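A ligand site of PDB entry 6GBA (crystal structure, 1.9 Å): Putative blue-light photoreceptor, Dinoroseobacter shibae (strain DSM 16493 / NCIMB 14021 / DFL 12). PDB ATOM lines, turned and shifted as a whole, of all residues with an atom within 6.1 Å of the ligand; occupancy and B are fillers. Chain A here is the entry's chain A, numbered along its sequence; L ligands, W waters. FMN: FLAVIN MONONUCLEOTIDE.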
ATOM      1  N   VAL A  38      -5.695 -20.803   4.527  1.00  0.00           N
ATOM      2  CA  VAL A  38      -4.866 -21.078   5.682  1.00  0.00           C
ATOM      3  C   VAL A  38      -5.342 -20.177   6.802  1.00  0.00           C
ATOM      4  O   VAL A  38      -5.663 -19.018   6.565  1.00  0.00           O
ATOM      5  CB  VAL A  38      -3.380 -20.803   5.373  1.00  0.00           C
ATOM      6  CG1 VAL A  38      -2.535 -20.978   6.626  1.00  0.00           C
ATOM      7  CG2 VAL A  38      -2.894 -21.689   4.228  1.00  0.00           C
ATOM      8  N   PHE A  39      -5.392 -20.708   8.036  1.00  0.00           N
ATOM      9  CA  PHE A  39      -5.479 -19.862   9.210  1.00  0.00           C
ATOM     10  C   PHE A  39      -4.201 -20.017  10.022  1.00  0.00           C
ATOM     11  O   PHE A  39      -3.719 -21.149  10.208  1.00  0.00           O
ATOM     12  CB  PHE A  39      -6.675 -20.199  10.103  1.00  0.00           C
ATOM     13  CG  PHE A  39      -7.992 -20.065   9.416  1.00  0.00           C
ATOM     14  CD1 PHE A  39      -8.564 -18.824   9.243  1.00  0.00           C
ATOM     15  CD2 PHE A  39      -8.651 -21.182   8.939  1.00  0.00           C
ATOM     16  CE1 PHE A  39      -9.781 -18.687   8.605  1.00  0.00           C
ATOM     17  CE2 PHE A  39      -9.869 -21.055   8.287  1.00  0.00           C
ATOM     18  CZ  PHE A  39     -10.424 -19.810   8.124  1.00  0.00           C
ATOM     19  N   SER A  40      -3.663 -18.900  10.485  1.00  0.00           N
ATOM     20  CA  SER A  40      -2.445 -18.883  11.270  1.00  0.00           C
ATOM     21  C   SER A  40      -2.758 -18.333  12.644  1.00  0.00           C
ATOM     22  O   SER A  40      -3.719 -17.592  12.842  1.00  0.00           O
ATOM     23  CB  SER A  40      -1.379 -18.017  10.609  1.00  0.00           C
ATOM     24  OG  SER A  40      -1.609 -16.626  10.877  1.00  0.00           O
ATOM     25  N   ASP A  46       6.360 -17.610  15.614  1.00  0.00           N
ATOM     26  CA  ASP A  46       6.524 -17.737  14.168  1.00  0.00           C
ATOM     27  C   ASP A  46       5.208 -17.857  13.414  1.00  0.00           C
ATOM     28  O   ASP A  46       5.200 -18.230  12.239  1.00  0.00           O
ATOM     29  CB  ASP A  46       7.440 -18.912  13.786  1.00  0.00           C
ATOM     30  CG  ASP A  46       8.189 -18.683  12.478  1.00  0.00           C
ATOM     31  OD1 ASP A  46       8.311 -17.502  12.056  1.00  0.00           O
ATOM     32  OD2 ASP A  46       8.659 -19.659  11.873  1.00  0.00           O
ATOM     33  N   ASN A  47       4.079 -17.510  14.046  1.00  0.00           N
ATOM     34  CA  ASN A  47       2.810 -17.331  13.357  1.00  0.00           C
ATOM     35  C   ASN A  47       2.451 -18.543  12.497  1.00  0.00           C
ATOM     36  O   ASN A  47       2.235 -18.419  11.281  1.00  0.00           O
ATOM     37  CB  ASN A  47       2.857 -16.054  12.521  1.00  0.00           C
ATOM     38  CG  ASN A  47       1.519 -15.709  11.868  1.00  0.00           C
ATOM     39  OD1 ASN A  47       1.499 -15.107  10.797  1.00  0.00           O
ATOM     40  ND2 ASN A  47       0.427 -16.080  12.499  1.00  0.00           N
ATOM     41  N   PHE A  56      -5.700 -26.278  -0.457  1.00  0.00           N
ATOM     42  CA  PHE A  56      -4.334 -25.797  -0.269  1.00  0.00           C
ATOM     43  C   PHE A  56      -3.332 -26.936  -0.419  1.00  0.00           C
ATOM     44  O   PHE A  56      -2.305 -26.798  -1.087  1.00  0.00           O
ATOM     45  CB  PHE A  56      -4.196 -25.134   1.101  1.00  0.00           C
ATOM     46  CG  PHE A  56      -2.788 -24.717   1.454  1.00  0.00           C
ATOM     47  CD1 PHE A  56      -1.906 -25.615   2.023  1.00  0.00           C
ATOM     48  CD2 PHE A  56      -2.380 -23.413   1.245  1.00  0.00           C
ATOM     49  CE1 PHE A  56      -0.617 -25.239   2.354  1.00  0.00           C
ATOM     50  CE2 PHE A  56      -1.091 -23.018   1.591  1.00  0.00           C
ATOM     51  CZ  PHE A  56      -0.208 -23.934   2.123  1.00  0.00           C
ATOM     52  N   ASN A  71       5.231 -21.883   9.736  1.00  0.00           N
ATOM     53  CA  ASN A  71       4.959 -20.622   9.046  1.00  0.00           C
ATOM     54  C   ASN A  71       4.852 -20.860   7.545  1.00  0.00           C
ATOM     55  O   ASN A  71       5.612 -21.644   6.965  1.00  0.00           O
ATOM     56  CB  ASN A  71       6.069 -19.617   9.357  1.00  0.00           C
ATOM     57  CG  ASN A  71       5.793 -18.249   8.756  1.00  0.00           C
ATOM     58  OD1 ASN A  71       5.988 -18.035   7.558  1.00  0.00           O
ATOM     59  ND2 ASN A  71       5.350 -17.307   9.605  1.00  0.00           N
ATOM     60  N   CYS A  72       3.918 -20.156   6.896  1.00  0.00           N
ATOM     61  CA  CYS A  72       3.654 -20.381   5.468  1.00  0.00           C
ATOM     62  C   CYS A  72       4.789 -19.934   4.556  1.00  0.00           C
ATOM     63  O   CYS A  72       4.636 -20.061   3.329  1.00  0.00           O
ATOM     64  CB  CYS A  72       2.377 -19.664   5.039  1.00  0.00           C
ATOM     65  SG  CYS A  72       0.929 -20.409   5.754  1.00  0.00           S
ATOM     66  N   ARG A  73       5.911 -19.421   5.073  1.00  0.00           N
ATOM     67  CA  ARG A  73       7.018 -19.078   4.194  1.00  0.00           C
ATOM     68  C   ARG A  73       7.587 -20.274   3.432  1.00  0.00           C
ATOM     69  O   ARG A  73       8.340 -20.073   2.472  1.00  0.00           O
ATOM     70  CB  ARG A  73       8.145 -18.422   5.006  1.00  0.00           C
ATOM     71  CG  ARG A  73       9.038 -19.439   5.668  1.00  0.00           C
ATOM     72  CD  ARG A  73      10.188 -18.768   6.369  1.00  0.00           C
ATOM     73  NE  ARG A  73       9.672 -17.790   7.315  1.00  0.00           N
ATOM     74  CZ  ARG A  73       9.363 -18.082   8.565  1.00  0.00           C
ATOM     75  NH1 ARG A  73       9.525 -19.323   9.023  1.00  0.00           N
ATOM     76  NH2 ARG A  73       8.898 -17.141   9.369  1.00  0.00           N
ATOM     77  N   LEU A  75       6.172 -21.816   1.321  1.00  0.00           N
ATOM     78  CA  LEU A  75       5.705 -21.674  -0.060  1.00  0.00           C
ATOM     79  C   LEU A  75       6.627 -20.821  -0.920  1.00  0.00           C
ATOM     80  O   LEU A  75       6.458 -20.787  -2.143  1.00  0.00           O
ATOM     81  CB  LEU A  75       4.306 -21.077  -0.064  1.00  0.00           C
ATOM     82  CG  LEU A  75       3.285 -21.946   0.665  1.00  0.00           C
ATOM     83  CD1 LEU A  75       1.980 -21.220   0.906  1.00  0.00           C
ATOM     84  CD2 LEU A  75       3.047 -23.237  -0.108  1.00  0.00           C
ATOM     85  N   GLN A  76       7.610 -20.145  -0.322  1.00  0.00           N
ATOM     86  CA  GLN A  76       8.497 -19.289  -1.097  1.00  0.00           C
ATOM     87  C   GLN A  76       9.693 -20.087  -1.577  1.00  0.00           C
ATOM     88  O   GLN A  76      10.071 -21.093  -0.996  1.00  0.00           O
ATOM     89  CB  GLN A  76       8.937 -18.084  -0.255  1.00  0.00           C
ATOM     90  CG  GLN A  76       7.729 -17.216   0.110  1.00  0.00           C
ATOM     91  CD  GLN A  76       7.874 -16.484   1.419  1.00  0.00           C
ATOM     92  OE1 GLN A  76       8.971 -16.345   1.968  1.00  0.00           O
ATOM     93  NE2 GLN A  76       6.750 -15.991   1.937  1.00  0.00           N
ATOM     94  N   THR A  80      11.324 -16.084  -5.516  1.00  0.00           N
ATOM     95  CA  THR A  80      10.348 -15.231  -4.847  1.00  0.00           C
ATOM     96  C   THR A  80      10.978 -13.865  -4.570  1.00  0.00           C
ATOM     97  O   THR A  80      12.136 -13.780  -4.174  1.00  0.00           O
ATOM     98  CB  THR A  80       9.880 -15.880  -3.560  1.00  0.00           C
ATOM     99  OG1 THR A  80       9.310 -17.153  -3.879  1.00  0.00           O
ATOM    100  CG2 THR A  80       8.825 -15.009  -2.858  1.00  0.00           C
ATOM    101  N   VAL A  85       7.976 -10.480   0.057  1.00  0.00           N
ATOM    102  CA  VAL A  85       7.961 -11.132   1.362  1.00  0.00           C
ATOM    103  C   VAL A  85       7.902 -10.074   2.460  1.00  0.00           C
ATOM    104  O   VAL A  85       7.133 -10.196   3.417  1.00  0.00           O
ATOM    105  CB  VAL A  85       9.180 -12.069   1.498  1.00  0.00           C
ATOM    106  CG1 VAL A  85       9.248 -12.706   2.882  1.00  0.00           C
ATOM    107  CG2 VAL A  85       9.127 -13.160   0.429  1.00  0.00           C
ATOM    108  N   GLU A  86       8.695  -9.016   2.330  1.00  0.00           N
ATOM    109  CA  GLU A  86       8.694  -7.977   3.350  1.00  0.00           C
ATOM    110  C   GLU A  86       7.360  -7.230   3.377  1.00  0.00           C
ATOM    111  O   GLU A  86       6.827  -6.934   4.450  1.00  0.00           O
ATOM    112  CB  GLU A  86       9.865  -7.026   3.123  1.00  0.00           C
ATOM    113  CG  GLU A  86      10.074  -6.000   4.232  1.00  0.00           C
ATOM    114  CD  GLU A  86      10.347  -6.639   5.579  1.00  0.00           C
ATOM    115  OE1 GLU A  86      10.913  -7.756   5.605  1.00  0.00           O
ATOM    116  OE2 GLU A  86      10.003  -6.029   6.621  1.00  0.00           O
ATOM    117  N   ILE A  88       4.435  -8.457   2.782  1.00  0.00           N
ATOM    118  CA  ILE A  88       3.508  -9.312   3.525  1.00  0.00           C
ATOM    119  C   ILE A  88       3.774  -9.185   5.013  1.00  0.00           C
ATOM    120  O   ILE A  88       2.838  -9.091   5.822  1.00  0.00           O
ATOM    121  CB  ILE A  88       3.651 -10.773   3.063  1.00  0.00           C
ATOM    122  CG1 ILE A  88       3.200 -10.943   1.612  1.00  0.00           C
ATOM    123  CG2 ILE A  88       2.848 -11.714   3.997  1.00  0.00           C
ATOM    124  CD1 ILE A  88       3.517 -12.370   1.049  1.00  0.00           C
ATOM    125  N   ARG A  89       5.052  -9.201   5.401  1.00  0.00           N
ATOM    126  CA  ARG A  89       5.399  -9.140   6.812  1.00  0.00           C
ATOM    127  C   ARG A  89       4.906  -7.838   7.430  1.00  0.00           C
ATOM    128  O   ARG A  89       4.364  -7.838   8.537  1.00  0.00           O
ATOM    129  CB  ARG A  89       6.904  -9.274   6.980  1.00  0.00           C
ATOM    130  CG  ARG A  89       7.348  -9.387   8.435  1.00  0.00           C
ATOM    131  CD  ARG A  89       8.861  -9.577   8.549  1.00  0.00           C
ATOM    132  NE  ARG A  89       9.550  -8.295   8.644  1.00  0.00           N
ATOM    133  CZ  ARG A  89       9.927  -7.724   9.783  1.00  0.00           C
ATOM    134  NH1 ARG A  89       9.685  -8.343  10.938  1.00  0.00           N
ATOM    135  NH2 ARG A  89      10.545  -6.547   9.775  1.00  0.00           N
ATOM    136  N   LEU A  92       1.099  -7.841   7.734  1.00  0.00           N
ATOM    137  CA  LEU A  92       0.676  -8.564   8.925  1.00  0.00           C
ATOM    138  C   LEU A  92       0.810  -7.705  10.177  1.00  0.00           C
ATOM    139  O   LEU A  92      -0.113  -7.640  10.996  1.00  0.00           O
ATOM    140  CB  LEU A  92       1.474  -9.866   9.070  1.00  0.00           C
ATOM    141  CG  LEU A  92       1.209 -10.909   7.986  1.00  0.00           C
ATOM    142  CD1 LEU A  92       2.202 -12.076   8.143  1.00  0.00           C
ATOM    143  CD2 LEU A  92      -0.219 -11.429   8.055  1.00  0.00           C
ATOM    144  N   ILE A 102       2.603 -13.005  -5.491  1.00  0.00           N
ATOM    145  CA  ILE A 102       3.930 -13.425  -5.087  1.00  0.00           C
ATOM    146  C   ILE A 102       4.189 -14.789  -5.720  1.00  0.00           C
ATOM    147  O   ILE A 102       3.288 -15.629  -5.824  1.00  0.00           O
ATOM    148  CB  ILE A 102       4.030 -13.462  -3.546  1.00  0.00           C
ATOM    149  CG1 ILE A 102       5.433 -13.826  -3.069  1.00  0.00           C
ATOM    150  CG2 ILE A 102       2.985 -14.401  -2.936  1.00  0.00           C
ATOM    151  CD1 ILE A 102       5.610 -13.665  -1.539  1.00  0.00           C
ATOM    152  N   LEU A 103       5.414 -14.987  -6.204  1.00  0.00           N
ATOM    153  CA  LEU A 103       5.775 -16.287  -6.774  1.00  0.00           C
ATOM    154  C   LEU A 103       5.925 -17.305  -5.660  1.00  0.00           C
ATOM    155  O   LEU A 103       6.669 -17.078  -4.688  1.00  0.00           O
ATOM    156  CB  LEU A 103       7.066 -16.170  -7.577  1.00  0.00           C
ATOM    157  CG  LEU A 103       7.444 -17.428  -8.345  1.00  0.00           C
ATOM    158  CD1 LEU A 103       6.493 -17.569  -9.526  1.00  0.00           C
ATOM    159  CD2 LEU A 103       8.864 -17.306  -8.789  1.00  0.00           C
ATOM    160  N   ASN A 104       5.202 -18.408  -5.767  1.00  0.00           N
ATOM    161  CA  ASN A 104       5.259 -19.483  -4.779  1.00  0.00           C
ATOM    162  C   ASN A 104       5.615 -20.783  -5.488  1.00  0.00           C
ATOM    163  O   ASN A 104       5.599 -20.883  -6.721  1.00  0.00           O
ATOM    164  CB  ASN A 104       3.936 -19.646  -4.025  1.00  0.00           C
ATOM    165  CG  ASN A 104       3.720 -18.609  -2.929  1.00  0.00           C
ATOM    166  OD1 ASN A 104       2.640 -18.578  -2.342  1.00  0.00           O
ATOM    167  ND2 ASN A 104       4.739 -17.795  -2.625  1.00  0.00           N
ATOM    168  N   ASN A 114       0.996 -16.594  -7.118  1.00  0.00           N
ATOM    169  CA  ASN A 114      -0.073 -16.708  -6.125  1.00  0.00           C
ATOM    170  C   ASN A 114      -0.605 -15.319  -5.813  1.00  0.00           C
ATOM    171  O   ASN A 114       0.150 -14.455  -5.344  1.00  0.00           O
ATOM    172  CB  ASN A 114       0.481 -17.368  -4.859  1.00  0.00           C
ATOM    173  CG  ASN A 114      -0.531 -17.466  -3.743  1.00  0.00           C
ATOM    174  OD1 ASN A 114      -1.738 -17.350  -3.961  1.00  0.00           O
ATOM    175  ND2 ASN A 114      -0.035 -17.680  -2.535  1.00  0.00           N
ATOM    176  N   LEU A 116      -2.254 -13.749  -3.196  1.00  0.00           N
ATOM    177  CA  LEU A 116      -2.457 -14.055  -1.795  1.00  0.00           C
ATOM    178  C   LEU A 116      -3.274 -12.948  -1.140  1.00  0.00           C
ATOM    179  O   LEU A 116      -2.904 -11.770  -1.225  1.00  0.00           O
ATOM    180  CB  LEU A 116      -1.109 -14.172  -1.088  1.00  0.00           C
ATOM    181  CG  LEU A 116      -1.137 -14.244   0.450  1.00  0.00           C
ATOM    182  CD1 LEU A 116      -1.844 -15.494   0.909  1.00  0.00           C
ATOM    183  CD2 LEU A 116       0.301 -14.246   0.943  1.00  0.00           C
ATOM    184  N   ILE A 118      -4.923 -11.714   2.517  1.00  0.00           N
ATOM    185  CA  ILE A 118      -4.791 -11.942   3.952  1.00  0.00           C
ATOM    186  C   ILE A 118      -5.688 -10.957   4.678  1.00  0.00           C
ATOM    187  O   ILE A 118      -5.846  -9.800   4.249  1.00  0.00           O
ATOM    188  CB  ILE A 118      -3.325 -11.819   4.406  1.00  0.00           C
ATOM    189  CG1 ILE A 118      -2.572 -13.113   4.054  1.00  0.00           C
ATOM    190  CG2 ILE A 118      -3.211 -11.506   5.905  1.00  0.00           C
ATOM    191  CD1 ILE A 118      -1.085 -13.046   4.256  1.00  0.00           C
ATOM    192  N   PHE A 131      -4.947 -14.922  11.589  1.00  0.00           N
ATOM    193  CA  PHE A 131      -4.936 -14.391  10.233  1.00  0.00           C
ATOM    194  C   PHE A 131      -5.560 -15.443   9.322  1.00  0.00           C
ATOM    195  O   PHE A 131      -5.361 -16.643   9.524  1.00  0.00           O
ATOM    196  CB  PHE A 131      -3.527 -14.093   9.754  1.00  0.00           C
ATOM    197  CG  PHE A 131      -2.944 -12.838  10.336  1.00  0.00           C
ATOM    198  CD1 PHE A 131      -3.391 -11.594   9.909  1.00  0.00           C
ATOM    199  CD2 PHE A 131      -1.956 -12.898  11.299  1.00  0.00           C
ATOM    200  CE1 PHE A 131      -2.857 -10.432  10.447  1.00  0.00           C
ATOM    201  CE2 PHE A 131      -1.409 -11.732  11.832  1.00  0.00           C
ATOM    202  CZ  PHE A 131      -1.861 -10.499  11.400  1.00  0.00           C
ATOM    203  N   ALA A 132      -6.339 -14.992   8.343  1.00  0.00           N
ATOM    204  CA  ALA A 132      -6.830 -15.871   7.286  1.00  0.00           C
ATOM    205  C   ALA A 132      -6.122 -15.490   6.014  1.00  0.00           C
ATOM    206  O   ALA A 132      -6.037 -14.317   5.685  1.00  0.00           O
ATOM    207  CB  ALA A 132      -8.340 -15.737   7.105  1.00  0.00           C
ATOM    208  N   GLY A 133      -5.596 -16.493   5.295  1.00  0.00           N
ATOM    209  CA  GLY A 133      -4.914 -16.276   4.031  1.00  0.00           C
ATOM    210  C   GLY A 133      -5.545 -17.151   2.974  1.00  0.00           C
ATOM    211  O   GLY A 133      -5.755 -18.350   3.201  1.00  0.00           O
ATOM    212  N   ALA A 134      -5.900 -16.572   1.845  1.00  0.00           N
ATOM    213  CA  ALA A 134      -6.475 -17.324   0.740  1.00  0.00           C
ATOM    214  C   ALA A 134      -5.537 -17.271  -0.456  1.00  0.00           C
ATOM    215  O   ALA A 134      -5.013 -16.197  -0.782  1.00  0.00           O
ATOM    216  CB  ALA A 134      -7.850 -16.763   0.365  1.00  0.00           C
ATOM    217  N   GLN A 135      -5.333 -18.410  -1.102  1.00  0.00           N
ATOM    218  CA  GLN A 135      -4.443 -18.509  -2.252  1.00  0.00           C
ATOM    219  C   GLN A 135      -5.260 -18.710  -3.528  1.00  0.00           C
ATOM    220  O   GLN A 135      -6.140 -19.581  -3.571  1.00  0.00           O
ATOM    221  CB  GLN A 135      -3.461 -19.668  -2.099  1.00  0.00           C
ATOM    222  CG  GLN A 135      -2.448 -19.472  -1.012  1.00  0.00           C
ATOM    223  CD  GLN A 135      -3.022 -19.792   0.351  1.00  0.00           C
ATOM    224  OE1 GLN A 135      -4.024 -20.503   0.486  1.00  0.00           O
ATOM    225  NE2 GLN A 135      -2.379 -19.266   1.384  1.00  0.00           N
HETATM  226  N1  FMN L   1       3.406 -16.449   1.984  1.00  0.00           N
HETATM  227  C2  FMN L   1       3.511 -16.959   0.699  1.00  0.00           C
HETATM  228  O2  FMN L   1       4.548 -16.758   0.050  1.00  0.00           O
HETATM  229  N3  FMN L   1       2.447 -17.653   0.172  1.00  0.00           N
HETATM  230  C4  FMN L   1       1.278 -17.854   0.892  1.00  0.00           C
HETATM  231  O4  FMN L   1       0.344 -18.483   0.397  1.00  0.00           O
HETATM  232  C4A FMN L   1       1.180 -17.353   2.190  1.00  0.00           C
HETATM  233  N5  FMN L   1       0.031 -17.562   2.941  1.00  0.00           N
HETATM  234  C5A FMN L   1      -0.044 -17.012   4.217  1.00  0.00           C
HETATM  235  C6  FMN L   1      -1.190 -17.180   4.989  1.00  0.00           C
HETATM  236  C7  FMN L   1      -1.261 -16.661   6.271  1.00  0.00           C
HETATM  237  C7M FMN L   1      -2.505 -16.848   7.082  1.00  0.00           C
HETATM  238  C8  FMN L   1      -0.185 -15.942   6.787  1.00  0.00           C
HETATM  239  C8M FMN L   1      -0.253 -15.357   8.164  1.00  0.00           C
HETATM  240  C9  FMN L   1       0.961 -15.754   6.029  1.00  0.00           C
HETATM  241  C9A FMN L   1       1.037 -16.293   4.746  1.00  0.00           C
HETATM  242  N10 FMN L   1       2.195 -16.134   3.999  1.00  0.00           N
HETATM  243  C10 FMN L   1       2.252 -16.637   2.715  1.00  0.00           C
HETATM  244  C1' FMN L   1       3.359 -15.327   4.487  1.00  0.00           C
HETATM  245  C2' FMN L   1       4.397 -16.010   5.362  1.00  0.00           C
HETATM  246  O2' FMN L   1       3.779 -16.829   6.311  1.00  0.00           O
HETATM  247  C3' FMN L   1       5.204 -14.911   6.044  1.00  0.00           C
HETATM  248  O3' FMN L   1       4.371 -14.079   6.824  1.00  0.00           O
HETATM  249  C4' FMN L   1       5.951 -14.080   5.002  1.00  0.00           C
HETATM  250  O4' FMN L   1       7.019 -14.860   4.496  1.00  0.00           O
HETATM  251  C5' FMN L   1       6.557 -12.809   5.576  1.00  0.00           C
HETATM  252  O5' FMN L   1       7.069 -13.107   6.854  1.00  0.00           O
HETATM  253  P   FMN L   1       8.628 -13.481   7.088  1.00  0.00           P
HETATM  254  O1P FMN L   1       8.988 -14.640   6.184  1.00  0.00           O
HETATM  255  O2P FMN L   1       9.505 -12.290   6.767  1.00  0.00           O
HETATM  256  O3P FMN L   1       8.819 -13.861   8.542  1.00  0.00           O
HETATM  257  O   HOH W   1       2.165 -18.247   8.343  1.00  0.00           O
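The side-chain amide nitrogen (NE2) of Gln 76 sits at hydrogen-bond distance from an oxygen (O4') of the ligand, at 2.8 Å. An oxygen (O3P) of the ligand lies within salt-bridge range of the guanidinium group (NH2) of Arg 73, at 3.4 Å. N3 of the ligand is in hydrogen-bond range of OD1 of Asn 104. The backbone NH (N) of Cys 72 lies within hydrogen-bond range of an oxygen (O2') of the ligand, 3.4 Å away. The side-chain amide nitrogen (NE2) of Gln 135 is in hydrogen-bond range of an oxygen (O4) of the ligand, 3.0 Å away. The side-chain amide nitrogen of Asn 114 lies within hydrogen-bond range of an oxygen (O4) of the ligand (3.1 Å). OD1 of Asn 71 is in hydrogen-bond range of O2' of the ligand.
OD1 of Asp 46 is in salt-bridge range of NH2 of Arg 73 (2.8 Å). The backbone carbonyl oxygen of Asp 46 lies within hydrogen-bond range of the side-chain amide nitrogen of Asn 71, 2.8 Å away. The side-chain hydroxyl (OG) of Ser 40 sits at hydrogen-bond distance from the side-chain amide nitrogen (ND2) of Asn 47 (2.7 Å). The backbone NH (N) of Ser 40 is in hydrogen-bond range of the backbone carbonyl oxygen (O) of Phe 131, 3.0 Å away. ND2 of Asn 104 lies close to O of Leu 75 (3.5 Å). The backbone carbonyl oxygen (O) of Gly 133 is in hydrogen-bond range of the backbone NH (N) of Val 38, at 2.8 Å. N of Arg 73 is in hydrogen-bond range of OD1 of Asn 71 (2.8 Å). ND2 of Asn 114 is in hydrogen-bond range of OD1 of Asn 104.
Val 38 touches the ligand (O to C7M, 3.9 Å). Ser 40 touches the ligand (OG to C8M, 3.3 Å). OD1 of Asn 47 touches C8M of the ligand (3.2 Å). CD1 of Leu 75 touches O4 of the ligand, 3.2 Å away. O of Val 85 touches C5' of the ligand, at 3.4 Å. Ile 88 touches the ligand. CD of Arg 89 touches O2P of the ligand, 3.3 Å away. Leu 92 touches the ligand. CD1 of Ile 102 touches O2 of the ligand, at 3.6 Å. Leu 116 touches the ligand. Ile 118 touches the ligand (CD1 to C9, 3.8 Å). O of Phe 131 touches C7M of the ligand, 3.8 Å away. Gly 133 touches the ligand (N to C7M, 3.6 Å). 20 residues have an atom within 4 Å of the ligand: Val 38, Ser 40, Asn 47, Asn 71, Cys 72, Arg 73, Leu 75, Gln 76, Val 85, Ile 88, Arg 89, Leu 92, Ile 102, Asn 104, Asn 114, Leu 116, Ile 118, Phe 131, Gly 133 and Gln 135. The nearest printed residue that does not touch the ligand is Ala 132 (4.01 Å).
Water W1 lies within hydrogen-bond range of the backbone carbonyl oxygen of Asn 47, an oxygen (O2') of the ligand and the backbone NH of Cys 72.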
